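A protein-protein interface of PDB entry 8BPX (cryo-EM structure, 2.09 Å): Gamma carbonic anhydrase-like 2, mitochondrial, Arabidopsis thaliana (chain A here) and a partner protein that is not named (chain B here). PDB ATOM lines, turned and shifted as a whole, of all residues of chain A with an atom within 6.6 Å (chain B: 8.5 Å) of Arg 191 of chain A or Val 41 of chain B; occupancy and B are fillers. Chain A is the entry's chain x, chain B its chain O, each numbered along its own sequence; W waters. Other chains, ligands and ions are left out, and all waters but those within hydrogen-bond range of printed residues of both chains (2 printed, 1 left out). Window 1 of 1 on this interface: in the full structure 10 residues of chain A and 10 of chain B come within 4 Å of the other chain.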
ATOM      1  N   THR A 131      18.675  15.227  21.227  1.00  0.00           N
ATOM      2  CA  THR A 131      19.422  13.975  21.277  1.00  0.00           C
ATOM      3  C   THR A 131      20.764  14.106  21.984  1.00  0.00           C
ATOM      4  O   THR A 131      21.375  13.081  22.300  1.00  0.00           O
ATOM      5  CB  THR A 131      19.663  13.446  19.861  1.00  0.00           C
ATOM      6  OG1 THR A 131      20.670  14.240  19.221  1.00  0.00           O
ATOM      7  CG2 THR A 131      18.385  13.513  19.043  1.00  0.00           C
ATOM      8  N   LEU A 133      23.491  15.087  20.614  1.00  0.00           N
ATOM      9  CA  LEU A 133      24.520  15.168  19.596  1.00  0.00           C
ATOM     10  C   LEU A 133      24.693  16.626  19.165  1.00  0.00           C
ATOM     11  O   LEU A 133      23.802  17.449  19.379  1.00  0.00           O
ATOM     12  CB  LEU A 133      24.145  14.274  18.413  1.00  0.00           C
ATOM     13  CG  LEU A 133      24.191  12.769  18.683  1.00  0.00           C
ATOM     14  CD1 LEU A 133      23.554  11.983  17.546  1.00  0.00           C
ATOM     15  CD2 LEU A 133      25.621  12.315  18.925  1.00  0.00           C
ATOM     16  N   GLY A 171      17.809  17.759  15.535  1.00  0.00           N
ATOM     17  CA  GLY A 171      18.400  16.488  15.887  1.00  0.00           C
ATOM     18  C   GLY A 171      17.964  15.314  15.042  1.00  0.00           C
ATOM     19  O   GLY A 171      18.383  14.184  15.324  1.00  0.00           O
ATOM     20  N   SER A 172      17.133  15.532  14.028  1.00  0.00           N
ATOM     21  CA  SER A 172      16.707  14.442  13.167  1.00  0.00           C
ATOM     22  C   SER A 172      17.856  13.995  12.265  1.00  0.00           C
ATOM     23  O   SER A 172      18.797  14.745  11.990  1.00  0.00           O
ATOM     24  CB  SER A 172      15.493  14.855  12.332  1.00  0.00           C
ATOM     25  OG  SER A 172      15.795  15.922  11.450  1.00  0.00           O
ATOM     26  N   LEU A 173      17.762  12.744  11.845  1.00  0.00           N
ATOM     27  CA  LEU A 173      18.823  12.118  11.031  1.00  0.00           C
ATOM     28  C   LEU A 173      18.301  11.314   9.829  1.00  0.00           C
ATOM     29  O   LEU A 173      17.432  10.523   9.976  1.00  0.00           O
ATOM     30  CB  LEU A 173      19.703  11.254  11.945  1.00  0.00           C
ATOM     31  CG  LEU A 173      20.701  10.339  11.234  1.00  0.00           C
ATOM     32  CD1 LEU A 173      21.868  11.152  10.676  1.00  0.00           C
ATOM     33  CD2 LEU A 173      21.193   9.244  12.164  1.00  0.00           C
ATOM     34  N   VAL A 174      18.794  11.634   8.669  1.00  0.00           N
ATOM     35  CA  VAL A 174      18.451  10.885   7.466  1.00  0.00           C
ATOM     36  C   VAL A 174      19.689  10.104   7.050  1.00  0.00           C
ATOM     37  O   VAL A 174      20.701  10.691   6.651  1.00  0.00           O
ATOM     38  CB  VAL A 174      17.959  11.798   6.336  1.00  0.00           C
ATOM     39  CG1 VAL A 174      17.481  10.966   5.159  1.00  0.00           C
ATOM     40  CG2 VAL A 174      16.841  12.694   6.832  1.00  0.00           C
ATOM     41  N   GLU A 175      19.568   8.795   7.167  1.00  0.00           N
ATOM     42  CA  GLU A 175      20.719   7.927   6.834  1.00  0.00           C
ATOM     43  C   GLU A 175      20.944   7.829   5.315  1.00  0.00           C
ATOM     44  O   GLU A 175      20.005   8.032   4.581  1.00  0.00           O
ATOM     45  CB  GLU A 175      20.577   6.564   7.516  1.00  0.00           C
ATOM     46  CG  GLU A 175      20.537   6.623   9.027  1.00  0.00           C
ATOM     47  CD  GLU A 175      20.325   5.273   9.693  1.00  0.00           C
ATOM     48  OE1 GLU A 175      20.268   4.236   8.986  1.00  0.00           O
ATOM     49  OE2 GLU A 175      20.230   5.259  10.907  1.00  0.00           O
ATOM     50  N   LEU A 186       9.454  15.316   9.580  1.00  0.00           N
ATOM     51  CA  LEU A 186      10.266  14.488  10.459  1.00  0.00           C
ATOM     52  C   LEU A 186      10.395  15.170  11.812  1.00  0.00           C
ATOM     53  O   LEU A 186      11.086  16.195  11.911  1.00  0.00           O
ATOM     54  CB  LEU A 186      11.644  14.240   9.848  1.00  0.00           C
ATOM     55  CG  LEU A 186      12.481  13.130  10.482  1.00  0.00           C
ATOM     56  CD1 LEU A 186      11.691  11.832  10.546  1.00  0.00           C
ATOM     57  CD2 LEU A 186      13.778  12.932   9.719  1.00  0.00           C
ATOM     58  N   PRO A 187       9.719  14.680  12.855  1.00  0.00           N
ATOM     59  CA  PRO A 187       9.792  15.346  14.142  1.00  0.00           C
ATOM     60  C   PRO A 187      11.196  15.313  14.792  1.00  0.00           C
ATOM     61  O   PRO A 187      11.971  14.551  14.441  1.00  0.00           O
ATOM     62  CB  PRO A 187       8.717  14.625  14.982  1.00  0.00           C
ATOM     63  CG  PRO A 187       7.842  13.909  13.983  1.00  0.00           C
ATOM     64  CD  PRO A 187       8.835  13.495  12.924  1.00  0.00           C
ATOM     65  N   GLY A 189      14.580  14.588  16.574  1.00  0.00           N
ATOM     66  CA  GLY A 189      15.260  13.388  17.012  1.00  0.00           C
ATOM     67  C   GLY A 189      14.841  12.111  16.324  1.00  0.00           C
ATOM     68  O   GLY A 189      15.273  11.035  16.741  1.00  0.00           O
ATOM     69  N   ARG A 190      13.996  12.188  15.299  1.00  0.00           N
ATOM     70  CA  ARG A 190      13.522  11.017  14.520  1.00  0.00           C
ATOM     71  C   ARG A 190      14.594  10.645  13.478  1.00  0.00           C
ATOM     72  O   ARG A 190      15.403  11.467  13.138  1.00  0.00           O
ATOM     73  CB  ARG A 190      12.101  11.164  13.957  1.00  0.00           C
ATOM     74  CG  ARG A 190      10.983  10.783  14.907  1.00  0.00           C
ATOM     75  CD  ARG A 190      10.981  11.582  16.188  1.00  0.00           C
ATOM     76  NE  ARG A 190       9.748  11.431  16.939  1.00  0.00           N
ATOM     77  CZ  ARG A 190       9.379  12.236  17.929  1.00  0.00           C
ATOM     78  NH1 ARG A 190      10.132  13.259  18.284  1.00  0.00           N
ATOM     79  NH2 ARG A 190       8.224  12.051  18.519  1.00  0.00           N
ATOM     80  N   ARG A 191      14.560   9.427  13.025  1.00  0.00           N
ATOM     81  CA  ARG A 191      15.568   8.875  12.118  1.00  0.00           C
ATOM     82  C   ARG A 191      14.933   8.202  10.896  1.00  0.00           C
ATOM     83  O   ARG A 191      13.970   7.503  11.036  1.00  0.00           O
ATOM     84  CB  ARG A 191      16.467   7.929  12.927  1.00  0.00           C
ATOM     85  CG  ARG A 191      17.385   6.997  12.159  1.00  0.00           C
ATOM     86  CD  ARG A 191      18.220   6.216  13.165  1.00  0.00           C
ATOM     87  NE  ARG A 191      17.500   5.208  13.913  1.00  0.00           N
ATOM     88  CZ  ARG A 191      17.363   3.942  13.529  1.00  0.00           C
ATOM     89  NH1 ARG A 191      17.899   3.528  12.398  1.00  0.00           N
ATOM     90  NH2 ARG A 191      16.670   3.110  14.269  1.00  0.00           N
ATOM     91  N   ILE A 192      15.523   8.403   9.772  1.00  0.00           N
ATOM     92  CA  ILE A 192      15.142   7.695   8.554  1.00  0.00           C
ATOM     93  C   ILE A 192      16.217   6.645   8.279  1.00  0.00           C
ATOM     94  O   ILE A 192      17.340   7.011   7.903  1.00  0.00           O
ATOM     95  CB  ILE A 192      14.977   8.647   7.364  1.00  0.00           C
ATOM     96  CG1 ILE A 192      14.052   9.813   7.723  1.00  0.00           C
ATOM     97  CG2 ILE A 192      14.442   7.890   6.155  1.00  0.00           C
ATOM     98  CD1 ILE A 192      12.634   9.393   8.033  1.00  0.00           C
ATOM     99  N   PRO A 193      15.929   5.359   8.453  1.00  0.00           N
ATOM    100  CA  PRO A 193      16.960   4.333   8.255  1.00  0.00           C
ATOM    101  C   PRO A 193      17.409   4.235   6.803  1.00  0.00           C
ATOM    102  O   PRO A 193      16.653   4.508   5.869  1.00  0.00           O
ATOM    103  CB  PRO A 193      16.270   3.040   8.712  1.00  0.00           C
ATOM    104  CG  PRO A 193      15.080   3.483   9.509  1.00  0.00           C
ATOM    105  CD  PRO A 193      14.659   4.790   8.926  1.00  0.00           C
ATOM    106  N   SER A 194      18.660   3.817   6.633  1.00  0.00           N
ATOM    107  CA  SER A 194      19.290   3.776   5.321  1.00  0.00           C
ATOM    108  C   SER A 194      18.561   2.824   4.377  1.00  0.00           C
ATOM    109  O   SER A 194      18.064   1.773   4.786  1.00  0.00           O
ATOM    110  CB  SER A 194      20.755   3.356   5.466  1.00  0.00           C
ATOM    111  OG  SER A 194      21.345   3.074   4.210  1.00  0.00           O
ATOM    112  N   TRP A 198      10.405   6.953   2.812  1.00  0.00           N
ATOM    113  CA  TRP A 198       9.519   7.399   3.877  1.00  0.00           C
ATOM    114  C   TRP A 198       8.682   8.576   3.390  1.00  0.00           C
ATOM    115  O   TRP A 198       9.007   9.224   2.392  1.00  0.00           O
ATOM    116  CB  TRP A 198      10.306   7.802   5.132  1.00  0.00           C
ATOM    117  CG  TRP A 198      10.756   6.652   5.971  1.00  0.00           C
ATOM    118  CD1 TRP A 198      11.528   5.604   5.574  1.00  0.00           C
ATOM    119  CD2 TRP A 198      10.480   6.444   7.361  1.00  0.00           C
ATOM    120  NE1 TRP A 198      11.741   4.748   6.627  1.00  0.00           N
ATOM    121  CE2 TRP A 198      11.109   5.241   7.736  1.00  0.00           C
ATOM    122  CE3 TRP A 198       9.759   7.156   8.324  1.00  0.00           C
ATOM    123  CZ2 TRP A 198      11.039   4.733   9.033  1.00  0.00           C
ATOM    124  CZ3 TRP A 198       9.686   6.648   9.608  1.00  0.00           C
ATOM    125  CH2 TRP A 198      10.327   5.452   9.953  1.00  0.00           C
ATOM    126  N   GLY B  37       9.054   8.613  16.311  1.00  0.00           N
ATOM    127  CA  GLY B  37       8.483   8.262  15.027  1.00  0.00           C
ATOM    128  C   GLY B  37       8.846   6.871  14.681  1.00  0.00           C
ATOM    129  O   GLY B  37       9.112   6.673  13.486  1.00  0.00           O
ATOM    130  N   SER B  38       8.801   5.957  15.656  1.00  0.00           N
ATOM    131  CA  SER B  38       9.045   4.520  15.539  1.00  0.00           C
ATOM    132  C   SER B  38      10.484   4.229  15.137  1.00  0.00           C
ATOM    133  O   SER B  38      10.929   3.078  15.193  1.00  0.00           O
ATOM    134  CB  SER B  38       8.076   3.875  14.546  1.00  0.00           C
ATOM    135  OG  SER B  38       8.366   2.500  14.372  1.00  0.00           O
ATOM    136  N   LYS B  39      11.225   5.268  14.760  1.00  0.00           N
ATOM    137  CA  LYS B  39      12.657   5.155  14.496  1.00  0.00           C
ATOM    138  C   LYS B  39      13.276   6.470  14.948  1.00  0.00           C
ATOM    139  O   LYS B  39      13.053   7.509  14.322  1.00  0.00           O
ATOM    140  CB  LYS B  39      12.948   4.880  13.022  1.00  0.00           C
ATOM    141  CG  LYS B  39      12.535   3.498  12.522  1.00  0.00           C
ATOM    142  CD  LYS B  39      13.353   2.392  13.169  1.00  0.00           C
ATOM    143  CE  LYS B  39      13.183   1.071  12.432  1.00  0.00           C
ATOM    144  NZ  LYS B  39      11.876   0.434  12.717  1.00  0.00           N
ATOM    145  N   LYS B  40      13.982   6.427  16.040  1.00  0.00           N
ATOM    146  CA  LYS B  40      14.637   7.568  16.642  1.00  0.00           C
ATOM    147  C   LYS B  40      16.158   7.449  16.662  1.00  0.00           C
ATOM    148  O   LYS B  40      16.700   6.348  16.739  1.00  0.00           O
ATOM    149  CB  LYS B  40      14.144   7.636  18.080  1.00  0.00           C
ATOM    150  CG  LYS B  40      12.641   7.892  18.203  1.00  0.00           C
ATOM    151  CD  LYS B  40      12.161   8.006  19.614  1.00  0.00           C
ATOM    152  CE  LYS B  40      11.079   9.040  19.865  1.00  0.00           C
ATOM    153  NZ  LYS B  40       9.786   8.680  19.250  1.00  0.00           N
ATOM    154  N   VAL B  41      16.785   8.606  16.774  1.00  0.00           N
ATOM    155  CA  VAL B  41      18.250   8.621  16.969  1.00  0.00           C
ATOM    156  C   VAL B  41      18.552   7.945  18.340  1.00  0.00           C
ATOM    157  O   VAL B  41      19.531   7.258  18.446  1.00  0.00           O
ATOM    158  CB  VAL B  41      18.772  10.062  16.855  1.00  0.00           C
ATOM    159  CG1 VAL B  41      20.266  10.144  17.138  1.00  0.00           C
ATOM    160  CG2 VAL B  41      18.422  10.728  15.531  1.00  0.00           C
ATOM    161  N   SER B  42      17.669   8.123  19.299  1.00  0.00           N
ATOM    162  CA  SER B  42      17.815   7.479  20.651  1.00  0.00           C
ATOM    163  C   SER B  42      17.970   5.952  20.537  1.00  0.00           C
ATOM    164  O   SER B  42      18.730   5.446  21.219  1.00  0.00           O
ATOM    165  CB  SER B  42      16.718   7.907  21.589  1.00  0.00           C
ATOM    166  OG  SER B  42      15.436   7.736  21.050  1.00  0.00           O
ATOM    167  N   ASP B  43      17.405   5.333  19.489  1.00  0.00           N
ATOM    168  CA  ASP B  43      17.582   3.869  19.256  1.00  0.00           C
ATOM    169  C   ASP B  43      19.049   3.499  18.997  1.00  0.00           C
ATOM    170  O   ASP B  43      19.389   2.321  19.221  1.00  0.00           O
ATOM    171  CB  ASP B  43      16.819   3.373  18.023  1.00  0.00           C
ATOM    172  CG  ASP B  43      15.342   3.724  17.949  1.00  0.00           C
ATOM    173  OD1 ASP B  43      14.754   4.046  18.991  1.00  0.00           O
ATOM    174  OD2 ASP B  43      14.790   3.663  16.833  1.00  0.00           O
ATOM    175  N   ARG B  44      19.886   4.440  18.543  1.00  0.00           N
ATOM    176  CA  ARG B  44      21.282   4.124  18.143  1.00  0.00           C
ATOM    177  C   ARG B  44      22.291   4.741  19.118  1.00  0.00           C
ATOM    178  O   ARG B  44      23.437   4.424  19.001  1.00  0.00           O
ATOM    179  CB  ARG B  44      21.520   4.626  16.718  1.00  0.00           C
ATOM    180  CG  ARG B  44      20.980   3.737  15.610  1.00  0.00           C
ATOM    181  CD  ARG B  44      21.352   4.337  14.272  1.00  0.00           C
ATOM    182  NE  ARG B  44      22.783   4.348  14.025  1.00  0.00           N
ATOM    183  CZ  ARG B  44      23.358   4.995  13.027  1.00  0.00           C
ATOM    184  NH1 ARG B  44      22.615   5.717  12.211  1.00  0.00           N
ATOM    185  NH2 ARG B  44      24.667   4.955  12.871  1.00  0.00           N
ATOM    186  N   ILE B  45      21.836   5.546  20.044  1.00  0.00           N
ATOM    187  CA  ILE B  45      22.726   6.266  20.987  1.00  0.00           C
ATOM    188  C   ILE B  45      23.372   5.261  21.944  1.00  0.00           C
ATOM    189  O   ILE B  45      22.720   4.373  22.414  1.00  0.00           O
ATOM    190  CB  ILE B  45      21.965   7.370  21.715  1.00  0.00           C
ATOM    191  CG1 ILE B  45      21.454   8.474  20.782  1.00  0.00           C
ATOM    192  CG2 ILE B  45      22.751   7.933  22.903  1.00  0.00           C
ATOM    193  CD1 ILE B  45      22.512   9.336  20.168  1.00  0.00           C
ATOM    194  N   VAL B  46      24.642   5.445  22.187  1.00  0.00           N
ATOM    195  CA  VAL B  46      25.379   4.524  23.089  1.00  0.00           C
ATOM    196  C   VAL B  46      25.966   5.349  24.227  1.00  0.00           C
ATOM    197  O   VAL B  46      26.710   6.283  23.887  1.00  0.00           O
ATOM    198  CB  VAL B  46      26.414   3.678  22.312  1.00  0.00           C
ATOM    199  CG1 VAL B  46      27.278   2.858  23.262  1.00  0.00           C
ATOM    200  CG2 VAL B  46      25.773   2.791  21.256  1.00  0.00           C
ATOM    201  N   LYS B  47      25.559   5.131  25.465  1.00  0.00           N
ATOM    202  CA  LYS B  47      26.038   5.866  26.631  1.00  0.00           C
ATOM    203  C   LYS B  47      27.480   5.463  26.920  1.00  0.00           C
ATOM    204  O   LYS B  47      27.797   4.271  26.966  1.00  0.00           O
ATOM    205  CB  LYS B  47      25.160   5.588  27.850  1.00  0.00           C
ATOM    206  CG  LYS B  47      24.059   6.604  28.145  1.00  0.00           C
ATOM    207  CD  LYS B  47      23.605   7.359  26.922  1.00  0.00           C
ATOM    208  CE  LYS B  47      22.500   8.350  27.266  1.00  0.00           C
ATOM    209  NZ  LYS B  47      21.955   9.031  26.060  1.00  0.00           N
ATOM    210  N   ILE B  61      28.471  10.756  24.246  1.00  0.00           N
ATOM    211  CA  ILE B  61      27.402  10.168  23.451  1.00  0.00           C
ATOM    212  C   ILE B  61      27.957   9.773  22.089  1.00  0.00           C
ATOM    213  O   ILE B  61      28.721  10.530  21.480  1.00  0.00           O
ATOM    214  CB  ILE B  61      26.228  11.162  23.298  1.00  0.00           C
ATOM    215  CG1 ILE B  61      25.384  11.172  24.566  1.00  0.00           C
ATOM    216  CG2 ILE B  61      25.346  10.788  22.127  1.00  0.00           C
ATOM    217  CD1 ILE B  61      25.084   9.814  25.075  1.00  0.00           C
ATOM    218  N   GLY B  62      27.608   8.592  21.596  1.00  0.00           N
ATOM    219  CA  GLY B  62      27.907   8.245  20.205  1.00  0.00           C
ATOM    220  C   GLY B  62      26.843   7.359  19.550  1.00  0.00           C
ATOM    221  O   GLY B  62      26.134   6.686  20.246  1.00  0.00           O
ATOM    222  N   LEU B  63      26.826   7.302  18.241  1.00  0.00           N
ATOM    223  CA  LEU B  63      25.932   6.342  17.537  1.00  0.00           C
ATOM    224  C   LEU B  63      26.533   4.960  17.372  1.00  0.00           C
ATOM    225  O   LEU B  63      27.707   4.862  17.085  1.00  0.00           O
ATOM    226  CB  LEU B  63      25.530   6.934  16.197  1.00  0.00           C
ATOM    227  CG  LEU B  63      24.767   8.257  16.248  1.00  0.00           C
ATOM    228  CD1 LEU B  63      24.489   8.778  14.851  1.00  0.00           C
ATOM    229  CD2 LEU B  63      23.479   8.120  17.042  1.00  0.00           C
ATOM    230  N   SER B  64      25.701   3.949  17.559  1.00  0.00           N
ATOM    231  CA  SER B  64      25.995   2.566  17.179  1.00  0.00           C
ATOM    232  C   SER B  64      26.287   2.513  15.671  1.00  0.00           C
ATOM    233  O   SER B  64      25.710   3.247  14.920  1.00  0.00           O
ATOM    234  CB  SER B  64      24.847   1.605  17.510  1.00  0.00           C
ATOM    235  OG  SER B  64      23.636   2.073  16.995  1.00  0.00           O
ATOM    236  N   GLN B 141      25.379  -1.655  20.924  1.00  0.00           N
ATOM    237  CA  GLN B 141      24.502  -1.592  22.135  1.00  0.00           C
ATOM    238  C   GLN B 141      25.205  -2.363  23.265  1.00  0.00           C
ATOM    239  O   GLN B 141      25.105  -1.950  24.405  1.00  0.00           O
ATOM    240  CB  GLN B 141      23.066  -2.076  21.753  1.00  0.00           C
ATOM    241  CG  GLN B 141      22.232  -1.069  20.980  1.00  0.00           C
ATOM    242  CD  GLN B 141      22.110   0.276  21.654  1.00  0.00           C
ATOM    243  OE1 GLN B 141      22.226   0.408  22.868  1.00  0.00           O
ATOM    244  NE2 GLN B 141      21.887   1.300  20.855  1.00  0.00           N
HETATM  245  O   HOH W   1       7.575  10.744  20.815  1.00  0.00           O
HETATM  246  O   HOH W   2      15.960  10.541  19.373  1.00  0.00           O
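Of the printed residues of chain B, Leu 173 of chain A touches Val 41 (3.8 Å) and Arg 44 (3.8 Å). Printed residues of chain B within 4 Å of Gly 189 of chain A: Lys 40 and Val 41. Of chain B, only Lys 39, Lys 40, Val 41, Asp 43 and Arg 44 come within 4 Å of Arg 191 of chain A. Of the printed residues of chain B, Pro 193 of chain A touches Lys 39 (3.9 Å). Val 41 of chain B touches just these residues of chain A: Leu 133, Gly 171, Leu 173, Gly 189, Arg 190 and Arg 191. Printed residues of chain A within 4 Å of Arg 44 of chain B: Leu 173 (3.8 Å), Glu 175 (2.8 Å) and Arg 191 (3.8 Å). The nearest residue of chain A that does not touch Val 41 of chain B is Thr 131 of chain A (4.1 Å). The nearest printed residue of chain B that does not touch Trp 198 of chain A is Ser 38 of chain B (5.3 Å).
O of Lys 39 of chain B lies within hydrogen-bond range of N of Arg 191 of chain A (2.8 Å). The backbone carbonyl oxygen of Lys 40 of chain B sits at hydrogen-bond distance from the guanidinium group of Arg 191 of chain A. The backbone carbonyl oxygen of Gly 189 of chain A is in hydrogen-bond range of the backbone NH of Val 41 of chain B, at 2.9 Å. The guanidinium group (NH2) of Arg 191 of chain A is in salt-bridge range of the side-chain carboxylate (OD2) of Asp 43 of chain B (3.2 Å). OE2 of Glu 175 of chain A lies within salt-bridge range of NH1 of Arg 44 of chain B (2.8 Å). N of Gly 37 of chain B sits close to NE of Arg 190 of chain A (3.0 Å).
Hydrophobic or aromatic side chains of chain A within 4 Å of the printed part of chain B: Leu 133, Leu 173, Pro 193 and Trp 198. Of the 16 printed residues of chain B, 9 touch a printed residue of chain A. Along chain B the printed residues that touch a printed residue of chain A span positions 37 to 63. Among the printed residues, 22 pairs touch across the chains.
Water W1 lies within hydrogen-bond range of NH2 of Arg 190 of chain A (2.7 Å) and NZ of Lys 40 of chain B (3.4 Å). Water W2 lies within hydrogen-bond range of O of Gly 189 of chain A (2.8 Å), N of Ser 42 of chain B (3.0 Å) and N of Val 41 of chain B (3.3 Å).
OD2 of Asp 43 of chain B lies within hydrogen-bond range of N of Lys 40 of chain B. N of Ser 64 of chain B lies within hydrogen-bond range of O of Arg 44 of chain B. OG1 of Thr 131 of chain A lies close to N of Leu 133 of chain A, 3.3 Å away. The backbone NH (N) of Leu 173 of chain A lies within hydrogen-bond range of the backbone carbonyl oxygen (O) of Arg 190 of chain A. O of Leu 173 of chain A lies within hydrogen-bond range of N of Ile 192 of chain A (2.9 Å). O of Ile 192 of chain A is in hydrogen-bond range of N of Glu 175 of chain A, 2.9 Å away.
Among the printed residues, pairs that only touch across the chains: Leu 133 of chain A with Val 41 of chain B, Leu 133 of chain A with Ile 45 of chain B, Leu 133 of chain A with Ile 61 of chain B, Leu 133 of chain A with Leu 63 of chain B, Gly 171 of chain A with Val 41 of chain B, Leu 173 of chain A with Val 41 of chain B, Leu 173 of chain A with Arg 44 of chain B, Gly 189 of chain A with Lys 40 of chain B, Arg 190 of chain A with Lys 39 of chain B, Arg 190 of chain A with Lys 40 of chain B, Arg 190 of chain A with Val 41 of chain B, Arg 191 of chain A with Val 41 of chain B, Arg 191 of chain A with Arg 44 of chain B, Pro 193 of chain A with Lys 39 of chain B, Trp 198 of chain A with Gly 37 of chain B and Trp 198 of chain A with Lys 39 of chain B.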
